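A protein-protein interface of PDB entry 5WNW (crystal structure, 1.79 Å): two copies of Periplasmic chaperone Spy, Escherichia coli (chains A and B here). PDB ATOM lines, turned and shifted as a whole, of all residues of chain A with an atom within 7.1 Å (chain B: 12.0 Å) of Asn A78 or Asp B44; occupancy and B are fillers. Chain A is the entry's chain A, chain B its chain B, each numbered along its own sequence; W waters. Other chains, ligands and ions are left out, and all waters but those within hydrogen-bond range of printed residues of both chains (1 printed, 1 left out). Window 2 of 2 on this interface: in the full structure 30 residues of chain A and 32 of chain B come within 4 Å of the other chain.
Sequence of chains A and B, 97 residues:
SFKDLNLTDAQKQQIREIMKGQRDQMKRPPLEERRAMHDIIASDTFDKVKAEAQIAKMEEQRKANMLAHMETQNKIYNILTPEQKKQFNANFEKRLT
Among the printed residues, pairs that only touch across the chains: Gln A73 with Ile B41, Asn A74 with Thr B45, Asn A74 with Phe B46, Tyr A77 with Ile B41, Tyr A77 with Ala B42 and Asn A78 with Asp B44.
Water W1 lies within hydrogen-bond range of OD1 of Asn A74 (2.9 Å), O of Asp B44 (3.0 Å) and ND2 of Asn A78 (3.2 Å).
O of Ile B40 is in hydrogen-bond range of ND2 of Asn A74 (3.2 Å). ND2 of Asn A74 is in hydrogen-bond range of O of Ile B41. The backbone carbonyl oxygen of Ser B43 lies within hydrogen-bond range of the side-chain amide nitrogen of Asn A74. The side-chain amide nitrogen of Asn A78 sits at hydrogen-bond distance from the backbone carbonyl oxygen of Ser B43 (3.0 Å).
No position is printed for both chains.
Of the printed residues of chain B, Asn A78 touches Ser B43 (3.0 Å) and Asp B44 (3.8 Å). Asn A74 touches five residues of chain B. No residue of chain B comes within 4 Å of Ile A76. Tyr A77 touches two residues of chain B. No residue of chain B comes within 4 Å of Ile A79. Of the printed residues of chain A, Ser B43 touches Asn A74 and Asn A78. Of the printed residues of chain A, Ala B42 touches Tyr A77. Printed residues of chain A within 4 Å of Thr B45: Asn A74. Printed residues of chain A within 4 Å of Ile B41: Gln A73 (3.9 Å), Asn A74 (2.9 Å) and Tyr A77 (3.7 Å). Of the printed residues of chain B, Gln A73 touches Ile B41. Met B37 touches none of the printed residues of chain A. Asp B39 touches none of the printed residues of chain A. The nearest residue of chain B that does not touch Asn A78 is Ile B41 (4.6 Å). The nearest residue of chain A that does not touch Asp B44 is Asn A74 (4.7 Å).
Of the 12 printed residues of chain A, 4 touch a printed residue of chain B. Hydrophobic or aromatic side chains of chain A within 4 Å of the printed part of chain B: Tyr A77. Printed residues of chain B that touch a printed residue of chain A: Ile B40, Ile B41, Ala B42, Ser B43, Asp B44, Thr B45 and Phe B46. Hydrophobic or aromatic side chains of chain B within 4 Å of the printed part of chain A: Ile B41, Ala B42 and Phe B46. Among the printed residues, 10 pairs touch across the chains.
The backbone carbonyl oxygen of Asn A74 sits at hydrogen-bond distance from the side-chain amide nitrogen of Asn A78 (3.0 Å). The side-chain hydroxyl of Ser B43 is in hydrogen-bond range of the backbone carbonyl oxygen of Thr B45, 2.8 Å away.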
ATOM      1  N   PHE A   2     -19.287  18.007 -14.155  1.00  0.00           N
ATOM      2  CA  PHE A   2     -18.233  17.892 -13.165  1.00  0.00           C
ATOM      3  C   PHE A   2     -18.186  19.076 -12.212  1.00  0.00           C
ATOM      4  O   PHE A   2     -17.727  18.928 -11.086  1.00  0.00           O
ATOM      5  CB  PHE A   2     -16.889  17.729 -13.857  1.00  0.00           C
ATOM      6  CG  PHE A   2     -16.746  16.420 -14.580  1.00  0.00           C
ATOM      7  CD1 PHE A   2     -17.120  15.234 -13.969  1.00  0.00           C
ATOM      8  CD2 PHE A   2     -16.256  16.379 -15.877  1.00  0.00           C
ATOM      9  CE1 PHE A   2     -16.996  14.032 -14.624  1.00  0.00           C
ATOM     10  CE2 PHE A   2     -16.127  15.175 -16.543  1.00  0.00           C
ATOM     11  CZ  PHE A   2     -16.504  13.997 -15.922  1.00  0.00           C
ATOM     12  N   THR A  72     -11.191  12.478 -22.485  1.00  0.00           N
ATOM     13  CA  THR A  72     -11.167  13.548 -21.477  1.00  0.00           C
ATOM     14  C   THR A  72     -12.127  13.253 -20.323  1.00  0.00           C
ATOM     15  O   THR A  72     -11.763  13.382 -19.147  1.00  0.00           O
ATOM     16  CB  THR A  72     -11.543  14.903 -22.120  1.00  0.00           C
ATOM     17  OG1 THR A  72     -10.530  15.249 -23.081  1.00  0.00           O
ATOM     18  CG2 THR A  72     -11.643  16.008 -21.075  1.00  0.00           C
ATOM     19  N   GLN A  73     -13.353  12.880 -20.661  1.00  0.00           N
ATOM     20  CA  GLN A  73     -14.363  12.524 -19.647  1.00  0.00           C
ATOM     21  C   GLN A  73     -13.907  11.352 -18.805  1.00  0.00           C
ATOM     22  O   GLN A  73     -14.049  11.348 -17.584  1.00  0.00           O
ATOM     23  CB  GLN A  73     -15.708  12.198 -20.292  1.00  0.00           C
ATOM     24  CG  GLN A  73     -16.345  13.340 -21.047  1.00  0.00           C
ATOM     25  CD  GLN A  73     -16.863  14.398 -20.084  1.00  0.00           C
ATOM     26  OE1 GLN A  73     -17.675  14.104 -19.214  1.00  0.00           O
ATOM     27  NE2 GLN A  73     -16.363  15.619 -20.215  1.00  0.00           N
ATOM     28  N   ASN A  74     -13.295  10.346 -19.452  1.00  0.00           N
ATOM     29  CA  ASN A  74     -12.771   9.235 -18.691  1.00  0.00           C
ATOM     30  C   ASN A  74     -11.633   9.660 -17.746  1.00  0.00           C
ATOM     31  O   ASN A  74     -11.596   9.225 -16.603  1.00  0.00           O
ATOM     32  CB  ASN A  74     -12.297   8.124 -19.639  1.00  0.00           C
ATOM     33  CG  ASN A  74     -11.700   6.948 -18.895  1.00  0.00           C
ATOM     34  OD1 ASN A  74     -10.493   6.840 -18.735  1.00  0.00           O
ATOM     35  ND2 ASN A  74     -12.546   6.044 -18.465  1.00  0.00           N
ATOM     36  N   LYS A  75     -10.776  10.569 -18.175  1.00  0.00           N
ATOM     37  CA  LYS A  75      -9.658  11.007 -17.314  1.00  0.00           C
ATOM     38  C   LYS A  75     -10.247  11.724 -16.122  1.00  0.00           C
ATOM     39  O   LYS A  75      -9.778  11.584 -14.987  1.00  0.00           O
ATOM     40  CB  LYS A  75      -8.701  11.927 -18.050  1.00  0.00           C
ATOM     41  CG  LYS A  75      -7.784  11.186 -19.047  1.00  0.00           C
ATOM     42  CD  LYS A  75      -6.856  12.169 -19.714  1.00  0.00           C
ATOM     43  CE  LYS A  75      -5.890  11.526 -20.682  1.00  0.00           C
ATOM     44  NZ  LYS A  75      -5.216  12.588 -21.463  1.00  0.00           N
ATOM     45  N   ILE A  76     -11.275  12.507 -16.378  1.00  0.00           N
ATOM     46  CA  ILE A  76     -11.804  13.335 -15.267  1.00  0.00           C
ATOM     47  C   ILE A  76     -12.546  12.424 -14.305  1.00  0.00           C
ATOM     48  O   ILE A  76     -12.429  12.529 -13.082  1.00  0.00           O
ATOM     49  CB  ILE A  76     -12.687  14.437 -15.755  1.00  0.00           C
ATOM     50  CG1 ILE A  76     -11.867  15.446 -16.559  1.00  0.00           C
ATOM     51  CG2 ILE A  76     -13.265  15.202 -14.555  1.00  0.00           C
ATOM     52  CD1 ILE A  76     -12.717  16.450 -17.319  1.00  0.00           C
ATOM     53  N   TYR A  77     -13.319  11.488 -14.856  1.00  0.00           N
ATOM     54  CA  TYR A  77     -14.035  10.570 -13.990  1.00  0.00           C
ATOM     55  C   TYR A  77     -13.054   9.890 -13.065  1.00  0.00           C
ATOM     56  O   TYR A  77     -13.327   9.735 -11.884  1.00  0.00           O
ATOM     57  CB  TYR A  77     -14.829   9.530 -14.812  1.00  0.00           C
ATOM     58  CG  TYR A  77     -15.552   8.487 -14.026  1.00  0.00           C
ATOM     59  CD1 TYR A  77     -16.866   8.676 -13.591  1.00  0.00           C
ATOM     60  CD2 TYR A  77     -14.939   7.310 -13.717  1.00  0.00           C
ATOM     61  CE1 TYR A  77     -17.538   7.689 -12.842  1.00  0.00           C
ATOM     62  CE2 TYR A  77     -15.580   6.313 -12.961  1.00  0.00           C
ATOM     63  CZ  TYR A  77     -16.891   6.502 -12.551  1.00  0.00           C
ATOM     64  OH  TYR A  77     -17.531   5.528 -11.804  1.00  0.00           O
ATOM     65  N   ASN A  78     -11.883   9.526 -13.568  1.00  0.00           N
ATOM     66  CA  ASN A  78     -10.969   8.777 -12.739  1.00  0.00           C
ATOM     67  C   ASN A  78     -10.198   9.611 -11.699  1.00  0.00           C
ATOM     68  O   ASN A  78      -9.458   9.034 -10.929  1.00  0.00           O
ATOM     69  CB  ASN A  78     -10.002   8.001 -13.598  1.00  0.00           C
ATOM     70  CG  ASN A  78     -10.588   6.688 -14.010  1.00  0.00           C
ATOM     71  OD1 ASN A  78     -10.712   5.781 -13.184  1.00  0.00           O
ATOM     72  ND2 ASN A  78     -11.014   6.589 -15.277  1.00  0.00           N
ATOM     73  N   ILE A  79     -10.357  10.925 -11.673  1.00  0.00           N
ATOM     74  CA  ILE A  79      -9.768  11.669 -10.523  1.00  0.00           C
ATOM     75  C   ILE A  79     -10.776  11.845  -9.387  1.00  0.00           C
ATOM     76  O   ILE A  79     -10.413  12.345  -8.301  1.00  0.00           O
ATOM     77  CB  ILE A  79      -9.212  13.095 -10.883  1.00  0.00           C
ATOM     78  CG1 ILE A  79     -10.338  14.084 -11.306  1.00  0.00           C
ATOM     79  CG2 ILE A  79      -8.075  13.014 -11.955  1.00  0.00           C
ATOM     80  CD1 ILE A  79      -9.877  15.471 -11.461  1.00  0.00           C
ATOM     81  N   LEU A  80     -12.036  11.495  -9.626  1.00  0.00           N
ATOM     82  CA  LEU A  80     -13.089  11.655  -8.610  1.00  0.00           C
ATOM     83  C   LEU A  80     -12.964  10.687  -7.451  1.00  0.00           C
ATOM     84  O   LEU A  80     -12.435   9.598  -7.602  1.00  0.00           O
ATOM     85  CB  LEU A  80     -14.461  11.465  -9.268  1.00  0.00           C
ATOM     86  CG  LEU A  80     -14.767  12.470 -10.365  1.00  0.00           C
ATOM     87  CD1 LEU A  80     -16.119  12.090 -10.987  1.00  0.00           C
ATOM     88  CD2 LEU A  80     -14.685  13.931  -9.845  1.00  0.00           C
ATOM     89  N   THR A  81     -13.431  11.087  -6.268  1.00  0.00           N
ATOM     90  CA  THR A  81     -13.570  10.153  -5.163  1.00  0.00           C
ATOM     91  C   THR A  81     -14.736   9.170  -5.388  1.00  0.00           C
ATOM     92  O   THR A  81     -15.609   9.407  -6.229  1.00  0.00           O
ATOM     93  CB  THR A  81     -13.820  10.909  -3.847  1.00  0.00           C
ATOM     94  OG1 THR A  81     -15.098  11.546  -3.937  1.00  0.00           O
ATOM     95  CG2 THR A  81     -12.761  11.927  -3.663  1.00  0.00           C
ATOM     96  N   LYS A  85     -18.018   9.867  -7.636  1.00  0.00           N
ATOM     97  CA  LYS A  85     -18.355   8.965  -8.720  1.00  0.00           C
ATOM     98  C   LYS A  85     -19.816   8.547  -8.665  1.00  0.00           C
ATOM     99  O   LYS A  85     -20.500   8.507  -9.704  1.00  0.00           O
ATOM    100  CB  LYS A  85     -17.468   7.723  -8.691  1.00  0.00           C
ATOM    101  CG  LYS A  85     -16.108   7.979  -9.312  1.00  0.00           C
ATOM    102  CD  LYS A  85     -15.223   6.744  -9.285  1.00  0.00           C
ATOM    103  CE  LYS A  85     -13.777   7.060  -9.676  1.00  0.00           C
ATOM    104  NZ  LYS A  85     -12.957   5.827  -9.478  1.00  0.00           N
ATOM    105  N   ALA B  36     -23.782   2.727 -23.418  1.00  0.00           N
ATOM    106  CA  ALA B  36     -22.443   2.358 -23.847  1.00  0.00           C
ATOM    107  C   ALA B  36     -21.477   3.508 -23.607  1.00  0.00           C
ATOM    108  O   ALA B  36     -20.343   3.306 -23.175  1.00  0.00           O
ATOM    109  CB  ALA B  36     -22.449   1.964 -25.334  1.00  0.00           C
ATOM    110  N   MET B  37     -21.938   4.727 -23.844  1.00  0.00           N
ATOM    111  CA  MET B  37     -21.122   5.890 -23.496  1.00  0.00           C
ATOM    112  C   MET B  37     -20.768   5.889 -22.019  1.00  0.00           C
ATOM    113  O   MET B  37     -19.632   6.206 -21.632  1.00  0.00           O
ATOM    114  CB  MET B  37     -21.849   7.176 -23.835  1.00  0.00           C
ATOM    115  CG  MET B  37     -21.013   8.416 -23.564  1.00  0.00           C
ATOM    116  SD  MET B  37     -19.872   8.696 -24.906  1.00  0.00           S
ATOM    117  CE  MET B  37     -18.840   9.915 -24.148  1.00  0.00           C
ATOM    118  N   HIS B  38     -21.742   5.548 -21.191  1.00  0.00           N
ATOM    119  CA  HIS B  38     -21.512   5.541 -19.764  1.00  0.00           C
ATOM    120  C   HIS B  38     -20.431   4.572 -19.386  1.00  0.00           C
ATOM    121  O   HIS B  38     -19.542   4.856 -18.581  1.00  0.00           O
ATOM    122  CB  HIS B  38     -22.782   5.179 -19.041  1.00  0.00           C
ATOM    123  CG  HIS B  38     -22.778   5.545 -17.594  1.00  0.00           C
ATOM    124  ND1 HIS B  38     -23.852   5.278 -16.784  1.00  0.00           N
ATOM    125  CD2 HIS B  38     -21.845   6.136 -16.799  1.00  0.00           C
ATOM    126  CE1 HIS B  38     -23.606   5.709 -15.560  1.00  0.00           C
ATOM    127  NE2 HIS B  38     -22.388   6.225 -15.539  1.00  0.00           N
ATOM    128  N   ASP B  39     -20.493   3.399 -19.959  1.00  0.00           N
ATOM    129  CA  ASP B  39     -19.512   2.395 -19.622  1.00  0.00           C
ATOM    130  C   ASP B  39     -18.098   2.774 -20.128  1.00  0.00           C
ATOM    131  O   ASP B  39     -17.115   2.379 -19.538  1.00  0.00           O
ATOM    132  CB  ASP B  39     -19.992   1.039 -20.164  1.00  0.00           C
ATOM    133  CG  ASP B  39     -21.242   0.548 -19.428  1.00  0.00           C
ATOM    134  OD1 ASP B  39     -21.547   1.121 -18.367  1.00  0.00           O
ATOM    135  OD2 ASP B  39     -21.945  -0.392 -19.863  1.00  0.00           O
ATOM    136  N   ILE B  40     -17.996   3.544 -21.212  1.00  0.00           N
ATOM    137  CA  ILE B  40     -16.694   4.011 -21.648  1.00  0.00           C
ATOM    138  C   ILE B  40     -16.122   5.039 -20.674  1.00  0.00           C
ATOM    139  O   ILE B  40     -14.946   4.990 -20.333  1.00  0.00           O
ATOM    140  CB  ILE B  40     -16.756   4.607 -23.058  1.00  0.00           C
ATOM    141  CG1 ILE B  40     -16.946   3.483 -24.063  1.00  0.00           C
ATOM    142  CG2 ILE B  40     -15.461   5.382 -23.372  1.00  0.00           C
ATOM    143  CD1 ILE B  40     -17.284   3.985 -25.441  1.00  0.00           C
ATOM    144  N   ILE B  41     -16.955   5.969 -20.207  1.00  0.00           N
ATOM    145  CA  ILE B  41     -16.496   7.012 -19.335  1.00  0.00           C
ATOM    146  C   ILE B  41     -16.113   6.478 -17.966  1.00  0.00           C
ATOM    147  O   ILE B  41     -15.106   6.873 -17.423  1.00  0.00           O
ATOM    148  CB  ILE B  41     -17.583   8.091 -19.142  1.00  0.00           C
ATOM    149  CG1 ILE B  41     -17.780   8.841 -20.438  1.00  0.00           C
ATOM    150  CG2 ILE B  41     -17.211   8.994 -17.991  1.00  0.00           C
ATOM    151  CD1 ILE B  41     -18.933   9.848 -20.390  1.00  0.00           C
ATOM    152  N   ALA B  42     -16.894   5.548 -17.418  1.00  0.00           N
ATOM    153  CA  ALA B  42     -16.668   5.079 -16.056  1.00  0.00           C
ATOM    154  C   ALA B  42     -15.636   3.915 -15.911  1.00  0.00           C
ATOM    155  O   ALA B  42     -15.413   3.395 -14.827  1.00  0.00           O
ATOM    156  CB  ALA B  42     -18.002   4.669 -15.435  1.00  0.00           C
ATOM    157  N   SER B  43     -14.939   3.581 -16.969  1.00  0.00           N
ATOM    158  CA  SER B  43     -13.959   2.510 -16.921  1.00  0.00           C
ATOM    159  C   SER B  43     -12.647   2.972 -16.250  1.00  0.00           C
ATOM    160  O   SER B  43     -12.313   4.149 -16.308  1.00  0.00           O
ATOM    161  CB  SER B  43     -13.700   2.011 -18.354  1.00  0.00           C
ATOM    162  OG  SER B  43     -12.608   1.133 -18.385  1.00  0.00           O
ATOM    163  N   ASP B  44     -11.908   2.053 -15.619  1.00  0.00           N
ATOM    164  CA  ASP B  44     -10.604   2.354 -15.031  1.00  0.00           C
ATOM    165  C   ASP B  44      -9.592   2.839 -16.065  1.00  0.00           C
ATOM    166  O   ASP B  44      -8.701   3.627 -15.769  1.00  0.00           O
ATOM    167  CB  ASP B  44     -10.030   1.123 -14.323  1.00  0.00           C
ATOM    168  CG  ASP B  44     -10.575   0.937 -12.925  1.00  0.00           C
ATOM    169  OD1 ASP B  44     -11.438   1.730 -12.477  1.00  0.00           O
ATOM    170  OD2 ASP B  44     -10.140  -0.026 -12.270  1.00  0.00           O
ATOM    171  N   THR B  45      -9.719   2.330 -17.284  1.00  0.00           N
ATOM    172  CA  THR B  45      -8.823   2.706 -18.363  1.00  0.00           C
ATOM    173  C   THR B  45      -9.634   3.162 -19.564  1.00  0.00           C
ATOM    174  O   THR B  45     -10.829   2.915 -19.632  1.00  0.00           O
ATOM    175  CB  THR B  45      -7.947   1.526 -18.777  1.00  0.00           C
ATOM    176  OG1 THR B  45      -8.750   0.342 -18.722  1.00  0.00           O
ATOM    177  CG2 THR B  45      -6.748   1.392 -17.840  1.00  0.00           C
ATOM    178  N   PHE B  46      -8.971   3.845 -20.486  1.00  0.00           N
ATOM    179  CA  PHE B  46      -9.574   4.216 -21.753  1.00  0.00           C
ATOM    180  C   PHE B  46      -9.061   3.269 -22.818  1.00  0.00           C
ATOM    181  O   PHE B  46      -7.858   3.156 -23.024  1.00  0.00           O
ATOM    182  CB  PHE B  46      -9.262   5.668 -22.088  1.00  0.00           C
ATOM    183  CG  PHE B  46      -9.886   6.131 -23.358  1.00  0.00           C
ATOM    184  CD1 PHE B  46     -11.244   6.308 -23.444  1.00  0.00           C
ATOM    185  CD2 PHE B  46      -9.112   6.365 -24.475  1.00  0.00           C
ATOM    186  CE1 PHE B  46     -11.817   6.734 -24.610  1.00  0.00           C
ATOM    187  CE2 PHE B  46      -9.696   6.777 -25.664  1.00  0.00           C
ATOM    188  CZ  PHE B  46     -11.040   6.968 -25.721  1.00  0.00           C
ATOM    189  N   ASP B  47      -9.998   2.579 -23.474  1.00  0.00           N
ATOM    190  CA  ASP B  47      -9.701   1.623 -24.511  1.00  0.00           C
ATOM    191  C   ASP B  47     -10.086   2.230 -25.844  1.00  0.00           C
ATOM    192  O   ASP B  47     -11.244   2.288 -26.168  1.00  0.00           O
ATOM    193  CB  ASP B  47     -10.475   0.321 -24.264  1.00  0.00           C
ATOM    194  CG  ASP B  47     -10.240  -0.739 -25.340  1.00  0.00           C
ATOM    195  OD1 ASP B  47      -9.734  -0.449 -26.456  1.00  0.00           O
ATOM    196  OD2 ASP B  47     -10.573  -1.911 -25.060  1.00  0.00           O
ATOM    197  N   LYS B  48      -9.109   2.646 -26.624  1.00  0.00           N
ATOM    198  CA  LYS B  48      -9.384   3.455 -27.785  1.00  0.00           C
ATOM    199  C   LYS B  48     -10.179   2.652 -28.824  1.00  0.00           C
ATOM    200  O   LYS B  48     -11.081   3.173 -29.473  1.00  0.00           O
ATOM    201  CB  LYS B  48      -8.079   3.949 -28.377  1.00  0.00           C
ATOM    202  CG  LYS B  48      -8.263   4.881 -29.520  1.00  0.00           C
ATOM    203  CD  LYS B  48      -7.050   5.731 -29.726  1.00  0.00           C
ATOM    204  CE  LYS B  48      -7.145   6.493 -31.028  1.00  0.00           C
ATOM    205  NZ  LYS B  48      -6.028   7.492 -31.123  1.00  0.00           N
ATOM    206  N   LYS B  50     -12.260   0.071 -28.347  1.00  0.00           N
ATOM    207  CA  LYS B  50     -13.637   0.009 -27.881  1.00  0.00           C
ATOM    208  C   LYS B  50     -14.384   1.326 -28.117  1.00  0.00           C
ATOM    209  O   LYS B  50     -15.532   1.352 -28.574  1.00  0.00           O
ATOM    210  CB  LYS B  50     -13.669  -0.313 -26.392  1.00  0.00           C
ATOM    211  CG  LYS B  50     -15.075  -0.654 -25.880  1.00  0.00           C
ATOM    212  CD  LYS B  50     -15.049  -1.339 -24.501  1.00  0.00           C
ATOM    213  CE  LYS B  50     -14.106  -2.545 -24.486  1.00  0.00           C
ATOM    214  NZ  LYS B  50     -14.180  -3.353 -25.782  1.00  0.00           N
HETATM  215  O   HOH W   1      -8.268   6.335 -16.907  1.00  0.00           O
